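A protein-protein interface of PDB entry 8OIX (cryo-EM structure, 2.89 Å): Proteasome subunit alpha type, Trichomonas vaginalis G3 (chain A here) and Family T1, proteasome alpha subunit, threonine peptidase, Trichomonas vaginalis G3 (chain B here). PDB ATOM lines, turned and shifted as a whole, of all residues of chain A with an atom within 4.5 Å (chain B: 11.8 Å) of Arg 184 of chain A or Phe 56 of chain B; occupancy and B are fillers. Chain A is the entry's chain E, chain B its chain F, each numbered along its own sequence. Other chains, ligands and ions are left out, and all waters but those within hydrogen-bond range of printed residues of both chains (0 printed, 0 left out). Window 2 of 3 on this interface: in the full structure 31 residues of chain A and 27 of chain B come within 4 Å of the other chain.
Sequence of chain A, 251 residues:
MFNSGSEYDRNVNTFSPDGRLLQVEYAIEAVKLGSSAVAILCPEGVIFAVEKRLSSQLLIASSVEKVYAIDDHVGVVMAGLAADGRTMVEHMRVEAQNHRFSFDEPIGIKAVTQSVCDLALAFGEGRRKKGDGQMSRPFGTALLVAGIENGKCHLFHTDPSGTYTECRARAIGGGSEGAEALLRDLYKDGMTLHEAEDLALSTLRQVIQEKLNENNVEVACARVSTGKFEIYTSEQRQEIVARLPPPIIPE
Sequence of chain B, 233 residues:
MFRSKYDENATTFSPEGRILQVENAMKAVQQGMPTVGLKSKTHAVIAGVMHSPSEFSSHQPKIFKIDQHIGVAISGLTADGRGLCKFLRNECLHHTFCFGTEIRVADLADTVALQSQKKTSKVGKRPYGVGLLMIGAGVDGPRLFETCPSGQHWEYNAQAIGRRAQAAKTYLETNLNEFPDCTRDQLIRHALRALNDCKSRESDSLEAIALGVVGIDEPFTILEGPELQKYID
The backbone NH (N) of Arg 168 of chain A sits at hydrogen-bond distance from the backbone carbonyl oxygen (O) of Phe 56 of chain B (2.6 Å).
The guanidinium group of Arg 184 of chain A is in salt-bridge range of the side-chain carboxylate of Glu 55 of chain B, 3.8 Å away.
O of Arg 168 of chain A sits at hydrogen-bond distance from OH of Tyr 187 of chain A (2.7 Å).
OG of Ser 52 of chain B is in hydrogen-bond range of O of Ser 54 of chain B (2.6 Å).
OG of Ser 52 of chain B sits at hydrogen-bond distance from O of Ser 57 of chain B (3.0 Å).
N of Ser 54 of chain B sits at hydrogen-bond distance from OG of Ser 57 of chain B (2.7 Å).
Among the printed residues, pairs that only touch across the chains: Cys 167 of chain A with Phe 56 of chain B, Cys 167 of chain A with Ser 57 of chain B, Ala 169 of chain A with Phe 56 of chain B, Glu 180 of chain A with Ser 54 of chain B, Leu 183 of chain A with Phe 56 of chain B, Arg 184 of chain A with Phe 56 of chain B and Tyr 187 of chain A with Phe 56 of chain B.
Arg 184 of chain A touches just these residues of chain B: Glu 55 (3.3 Å) and Phe 56 (3.2 Å).
Phe 56 of chain B touches six residues of chain A.
Cys 167 of chain A touches just these residues of chain B: Phe 56 (3.5 Å) and Ser 57 (3.7 Å).
Arg 168 of chain A touches just one residue of chain B: Phe 56.
Ala 169 of chain A touches just one residue of chain B: Phe 56.
Glu 180 of chain A touches just one residue of chain B: Ser 54.
Ala 181 of chain A touches none of the printed residues of chain B.
No residue of chain B comes within 4 Å of Leu 186 of chain A.
Printed residues of chain A within 4 Å of Ser 54 of chain B: Glu 180 (3.96 Å).
Printed residues of chain A within 4 Å of Glu 55 of chain B: Arg 184.
Of the printed residues of chain A, Ser 57 of chain B touches Cys 167.
The nearest printed residue of chain A that does not touch Phe 56 of chain B is Glu 180 of chain A (4.5 Å).
The nearest printed residue of chain A that does not touch Glu 55 of chain B is Arg 168 of chain A (4.1 Å).
Hydrophobic or aromatic side chains of chain B within 4 Å of the printed part of chain A: Phe 56.
Of the 11 printed residues of chain A, 7 touch a printed residue of chain B.
Among the printed residues, Asp or Glu carboxylates within 4 Å of a Lys or Arg side-chain nitrogen of the other chain: Arg 184 of chain A with Glu 55 of chain B (3.8 Å).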
ATOM      1  N   CYS A 167      36.054  31.529  24.841  1.00  0.00           N
ATOM      2  CA  CYS A 167      34.993  30.557  25.057  1.00  0.00           C
ATOM      3  C   CYS A 167      34.804  30.289  26.541  1.00  0.00           C
ATOM      4  O   CYS A 167      35.774  30.128  27.284  1.00  0.00           O
ATOM      5  CB  CYS A 167      35.290  29.239  24.335  1.00  0.00           C
ATOM      6  SG  CYS A 167      35.708  29.418  22.593  1.00  0.00           S
ATOM      7  N   ARG A 168      33.542  30.254  26.966  1.00  0.00           N
ATOM      8  CA  ARG A 168      33.215  29.703  28.272  1.00  0.00           C
ATOM      9  C   ARG A 168      33.240  28.180  28.237  1.00  0.00           C
ATOM     10  O   ARG A 168      33.601  27.535  29.226  1.00  0.00           O
ATOM     11  CB  ARG A 168      31.849  30.214  28.728  1.00  0.00           C
ATOM     12  CG  ARG A 168      31.728  31.725  28.768  1.00  0.00           C
ATOM     13  CD  ARG A 168      30.370  32.170  28.256  1.00  0.00           C
ATOM     14  NE  ARG A 168      29.279  31.510  28.960  1.00  0.00           N
ATOM     15  CZ  ARG A 168      27.996  31.669  28.670  1.00  0.00           C
ATOM     16  NH1 ARG A 168      27.603  32.461  27.686  1.00  0.00           N
ATOM     17  NH2 ARG A 168      27.083  31.016  29.383  1.00  0.00           N
ATOM     18  N   ALA A 169      32.849  27.593  27.109  1.00  0.00           N
ATOM     19  CA  ALA A 169      32.947  26.157  26.897  1.00  0.00           C
ATOM     20  C   ALA A 169      33.104  25.912  25.407  1.00  0.00           C
ATOM     21  O   ALA A 169      32.493  26.608  24.591  1.00  0.00           O
ATOM     22  CB  ALA A 169      31.720  25.418  27.436  1.00  0.00           C
ATOM     23  N   GLU A 180      29.294  20.022  21.595  1.00  0.00           N
ATOM     24  CA  GLU A 180      28.674  21.330  21.785  1.00  0.00           C
ATOM     25  C   GLU A 180      27.182  21.195  22.053  1.00  0.00           C
ATOM     26  O   GLU A 180      26.628  21.895  22.913  1.00  0.00           O
ATOM     27  CB  GLU A 180      28.915  22.214  20.561  1.00  0.00           C
ATOM     28  CG  GLU A 180      30.350  22.689  20.384  1.00  0.00           C
ATOM     29  CD  GLU A 180      30.771  23.711  21.419  1.00  0.00           C
ATOM     30  OE1 GLU A 180      29.907  24.201  22.176  1.00  0.00           O
ATOM     31  OE2 GLU A 180      31.976  24.034  21.468  1.00  0.00           O
ATOM     32  N   ALA A 181      26.513  20.296  21.328  1.00  0.00           N
ATOM     33  CA  ALA A 181      25.092  20.065  21.565  1.00  0.00           C
ATOM     34  C   ALA A 181      24.845  19.578  22.987  1.00  0.00           C
ATOM     35  O   ALA A 181      23.895  20.017  23.646  1.00  0.00           O
ATOM     36  CB  ALA A 181      24.545  19.063  20.550  1.00  0.00           C
ATOM     37  N   LEU A 182      25.680  18.658  23.471  1.00  0.00           N
ATOM     38  CA  LEU A 182      25.546  18.190  24.847  1.00  0.00           C
ATOM     39  C   LEU A 182      25.839  19.301  25.847  1.00  0.00           C
ATOM     40  O   LEU A 182      25.200  19.382  26.902  1.00  0.00           O
ATOM     41  CB  LEU A 182      26.469  16.997  25.084  1.00  0.00           C
ATOM     42  CG  LEU A 182      26.137  15.765  24.243  1.00  0.00           C
ATOM     43  CD1 LEU A 182      27.266  14.766  24.314  1.00  0.00           C
ATOM     44  CD2 LEU A 182      24.833  15.138  24.707  1.00  0.00           C
ATOM     45  N   LEU A 183      26.805  20.167  25.536  1.00  0.00           N
ATOM     46  CA  LEU A 183      27.123  21.284  26.418  1.00  0.00           C
ATOM     47  C   LEU A 183      26.029  22.339  26.445  1.00  0.00           C
ATOM     48  O   LEU A 183      25.976  23.118  27.401  1.00  0.00           O
ATOM     49  CB  LEU A 183      28.446  21.932  26.007  1.00  0.00           C
ATOM     50  CG  LEU A 183      29.714  21.096  26.181  1.00  0.00           C
ATOM     51  CD1 LEU A 183      30.931  21.843  25.659  1.00  0.00           C
ATOM     52  CD2 LEU A 183      29.893  20.715  27.637  1.00  0.00           C
ATOM     53  N   ARG A 184      25.169  22.380  25.421  1.00  0.00           N
ATOM     54  CA  ARG A 184      24.096  23.369  25.354  1.00  0.00           C
ATOM     55  C   ARG A 184      23.366  23.507  26.686  1.00  0.00           C
ATOM     56  O   ARG A 184      23.321  24.591  27.278  1.00  0.00           O
ATOM     57  CB  ARG A 184      23.111  22.994  24.244  1.00  0.00           C
ATOM     58  CG  ARG A 184      23.557  23.365  22.841  1.00  0.00           C
ATOM     59  CD  ARG A 184      23.345  24.845  22.570  1.00  0.00           C
ATOM     60  NE  ARG A 184      23.844  25.236  21.257  1.00  0.00           N
ATOM     61  CZ  ARG A 184      23.666  26.433  20.715  1.00  0.00           C
ATOM     62  NH1 ARG A 184      22.981  27.379  21.336  1.00  0.00           N
ATOM     63  NH2 ARG A 184      24.182  26.685  19.514  1.00  0.00           N
ATOM     64  N   ASP A 185      22.785  22.413  27.174  1.00  0.00           N
ATOM     65  CA  ASP A 185      21.980  22.434  28.387  1.00  0.00           C
ATOM     66  C   ASP A 185      22.732  21.921  29.609  1.00  0.00           C
ATOM     67  O   ASP A 185      22.125  21.754  30.672  1.00  0.00           O
ATOM     68  CB  ASP A 185      20.704  21.616  28.182  1.00  0.00           C
ATOM     69  CG  ASP A 185      20.958  20.317  27.443  1.00  0.00           C
ATOM     70  OD1 ASP A 185      22.071  20.147  26.903  1.00  0.00           O
ATOM     71  OD2 ASP A 185      20.045  19.467  27.405  1.00  0.00           O
ATOM     72  N   LEU A 186      24.037  21.669  29.486  1.00  0.00           N
ATOM     73  CA  LEU A 186      24.830  21.141  30.588  1.00  0.00           C
ATOM     74  C   LEU A 186      25.821  22.133  31.178  1.00  0.00           C
ATOM     75  O   LEU A 186      26.321  21.892  32.280  1.00  0.00           O
ATOM     76  CB  LEU A 186      25.596  19.885  30.144  1.00  0.00           C
ATOM     77  CG  LEU A 186      24.897  18.520  30.193  1.00  0.00           C
ATOM     78  CD1 LEU A 186      24.739  18.066  31.635  1.00  0.00           C
ATOM     79  CD2 LEU A 186      23.549  18.524  29.487  1.00  0.00           C
ATOM     80  N   TYR A 187      26.113  23.232  30.489  1.00  0.00           N
ATOM     81  CA  TYR A 187      27.146  24.166  30.914  1.00  0.00           C
ATOM     82  C   TYR A 187      26.522  25.410  31.534  1.00  0.00           C
ATOM     83  O   TYR A 187      25.585  25.988  30.973  1.00  0.00           O
ATOM     84  CB  TYR A 187      28.037  24.569  29.739  1.00  0.00           C
ATOM     85  CG  TYR A 187      29.105  25.561  30.128  1.00  0.00           C
ATOM     86  CD1 TYR A 187      30.258  25.148  30.771  1.00  0.00           C
ATOM     87  CD2 TYR A 187      28.947  26.914  29.875  1.00  0.00           C
ATOM     88  CE1 TYR A 187      31.229  26.051  31.139  1.00  0.00           C
ATOM     89  CE2 TYR A 187      29.912  27.824  30.241  1.00  0.00           C
ATOM     90  CZ  TYR A 187      31.051  27.386  30.873  1.00  0.00           C
ATOM     91  OH  TYR A 187      32.023  28.285  31.242  1.00  0.00           O
ATOM     92  N   HIS B  51      30.563  38.050  15.645  1.00  0.00           N
ATOM     93  CA  HIS B  51      30.151  36.675  15.406  1.00  0.00           C
ATOM     94  C   HIS B  51      30.506  35.803  16.601  1.00  0.00           C
ATOM     95  O   HIS B  51      31.619  35.883  17.131  1.00  0.00           O
ATOM     96  CB  HIS B  51      30.811  36.127  14.141  1.00  0.00           C
ATOM     97  CG  HIS B  51      30.465  34.699  13.852  1.00  0.00           C
ATOM     98  ND1 HIS B  51      31.422  33.722  13.681  1.00  0.00           N
ATOM     99  CD2 HIS B  51      29.269  34.082  13.714  1.00  0.00           C
ATOM    100  CE1 HIS B  51      30.829  32.566  13.445  1.00  0.00           C
ATOM    101  NE2 HIS B  51      29.522  32.757  13.459  1.00  0.00           N
ATOM    102  N   SER B  52      29.554  34.974  17.021  1.00  0.00           N
ATOM    103  CA  SER B  52      29.764  34.014  18.099  1.00  0.00           C
ATOM    104  C   SER B  52      29.693  32.609  17.521  1.00  0.00           C
ATOM    105  O   SER B  52      28.591  32.087  17.292  1.00  0.00           O
ATOM    106  CB  SER B  52      28.718  34.198  19.201  1.00  0.00           C
ATOM    107  OG  SER B  52      28.856  33.212  20.209  1.00  0.00           O
ATOM    108  N   PRO B  53      30.830  31.961  17.251  1.00  0.00           N
ATOM    109  CA  PRO B  53      30.786  30.633  16.616  1.00  0.00           C
ATOM    110  C   PRO B  53      30.043  29.590  17.430  1.00  0.00           C
ATOM    111  O   PRO B  53      29.420  28.693  16.847  1.00  0.00           O
ATOM    112  CB  PRO B  53      32.270  30.271  16.453  1.00  0.00           C
ATOM    113  CG  PRO B  53      32.989  31.145  17.416  1.00  0.00           C
ATOM    114  CD  PRO B  53      32.206  32.410  17.507  1.00  0.00           C
ATOM    115  N   SER B  54      30.084  29.678  18.756  1.00  0.00           N
ATOM    116  CA  SER B  54      29.422  28.719  19.625  1.00  0.00           C
ATOM    117  C   SER B  54      28.565  29.467  20.638  1.00  0.00           C
ATOM    118  O   SER B  54      28.696  30.680  20.823  1.00  0.00           O
ATOM    119  CB  SER B  54      30.436  27.819  20.342  1.00  0.00           C
ATOM    120  OG  SER B  54      31.456  27.399  19.455  1.00  0.00           O
ATOM    121  N   GLU B  55      27.667  28.723  21.287  1.00  0.00           N
ATOM    122  CA  GLU B  55      26.784  29.325  22.281  1.00  0.00           C
ATOM    123  C   GLU B  55      27.579  29.913  23.440  1.00  0.00           C
ATOM    124  O   GLU B  55      27.341  31.052  23.857  1.00  0.00           O
ATOM    125  CB  GLU B  55      25.784  28.282  22.786  1.00  0.00           C
ATOM    126  CG  GLU B  55      25.127  28.597  24.131  1.00  0.00           C
ATOM    127  CD  GLU B  55      24.418  29.944  24.179  1.00  0.00           C
ATOM    128  OE1 GLU B  55      24.099  30.510  23.112  1.00  0.00           O
ATOM    129  OE2 GLU B  55      24.181  30.442  25.301  1.00  0.00           O
ATOM    130  N   PHE B  56      28.532  29.152  23.969  1.00  0.00           N
ATOM    131  CA  PHE B  56      29.331  29.589  25.105  1.00  0.00           C
ATOM    132  C   PHE B  56      30.631  30.259  24.694  1.00  0.00           C
ATOM    133  O   PHE B  56      31.416  30.642  25.567  1.00  0.00           O
ATOM    134  CB  PHE B  56      29.613  28.403  26.024  1.00  0.00           C
ATOM    135  CG  PHE B  56      28.393  27.600  26.338  1.00  0.00           C
ATOM    136  CD1 PHE B  56      27.386  28.132  27.123  1.00  0.00           C
ATOM    137  CD2 PHE B  56      28.235  26.327  25.825  1.00  0.00           C
ATOM    138  CE1 PHE B  56      26.254  27.401  27.408  1.00  0.00           C
ATOM    139  CE2 PHE B  56      27.106  25.594  26.105  1.00  0.00           C
ATOM    140  CZ  PHE B  56      26.113  26.132  26.897  1.00  0.00           C
ATOM    141  N   SER B  57      30.882  30.405  23.399  1.00  0.00           N
ATOM    142  CA  SER B  57      32.020  31.184  22.949  1.00  0.00           C
ATOM    143  C   SER B  57      31.658  32.662  22.940  1.00  0.00           C
ATOM    144  O   SER B  57      30.521  33.044  22.657  1.00  0.00           O
ATOM    145  CB  SER B  57      32.460  30.743  21.552  1.00  0.00           C
ATOM    146  OG  SER B  57      31.520  31.145  20.574  1.00  0.00           O
ATOM    147  N   SER B  58      32.641  33.497  23.260  1.00  0.00           N
ATOM    148  CA  SER B  58      32.427  34.931  23.204  1.00  0.00           C
ATOM    149  C   SER B  58      32.298  35.383  21.755  1.00  0.00           C
ATOM    150  O   SER B  58      32.652  34.665  20.816  1.00  0.00           O
ATOM    151  CB  SER B  58      33.569  35.681  23.888  1.00  0.00           C
ATOM    152  OG  SER B  58      33.573  35.442  25.284  1.00  0.00           O
ATOM    153  N   HIS B  59      31.777  36.589  21.579  1.00  0.00           N
ATOM    154  CA  HIS B  59      31.680  37.171  20.252  1.00  0.00           C
ATOM    155  C   HIS B  59      33.060  37.614  19.791  1.00  0.00           C
ATOM    156  O   HIS B  59      33.764  38.334  20.505  1.00  0.00           O
ATOM    157  CB  HIS B  59      30.704  38.345  20.259  1.00  0.00           C
ATOM    158  CG  HIS B  59      29.339  37.986  20.758  1.00  0.00           C
ATOM    159  ND1 HIS B  59      28.291  37.694  19.913  1.00  0.00           N
ATOM    160  CD2 HIS B  59      28.853  37.868  22.015  1.00  0.00           C
ATOM    161  CE1 HIS B  59      27.218  37.411  20.628  1.00  0.00           C
ATOM    162  NE2 HIS B  59      27.531  37.511  21.907  1.00  0.00           N
ATOM    163  N   GLN B  60      33.447  37.168  18.602  1.00  0.00           N
ATOM    164  CA  GLN B  60      34.775  37.459  18.087  1.00  0.00           C
ATOM    165  C   GLN B  60      34.923  38.960  17.861  1.00  0.00           C
ATOM    166  O   GLN B  60      34.060  39.568  17.215  1.00  0.00           O
ATOM    167  CB  GLN B  60      35.016  36.699  16.785  1.00  0.00           C
ATOM    168  CG  GLN B  60      34.945  35.195  16.947  1.00  0.00           C
ATOM    169  CD  GLN B  60      35.173  34.452  15.650  1.00  0.00           C
ATOM    170  OE1 GLN B  60      36.288  34.034  15.354  1.00  0.00           O
ATOM    171  NE2 GLN B  60      34.114  34.287  14.868  1.00  0.00           N
ATOM    172  N   GLU B 207      24.785  42.491  23.192  1.00  0.00           N
ATOM    173  CA  GLU B 207      26.062  41.912  23.582  1.00  0.00           C
ATOM    174  C   GLU B 207      26.890  41.454  22.392  1.00  0.00           C
ATOM    175  O   GLU B 207      28.065  41.112  22.565  1.00  0.00           O
ATOM    176  CB  GLU B 207      25.837  40.731  24.532  1.00  0.00           C
ATOM    177  CG  GLU B 207      24.927  41.052  25.704  1.00  0.00           C
ATOM    178  CD  GLU B 207      25.429  42.219  26.528  1.00  0.00           C
ATOM    179  OE1 GLU B 207      26.549  42.125  27.074  1.00  0.00           O
ATOM    180  OE2 GLU B 207      24.705  43.230  26.627  1.00  0.00           O
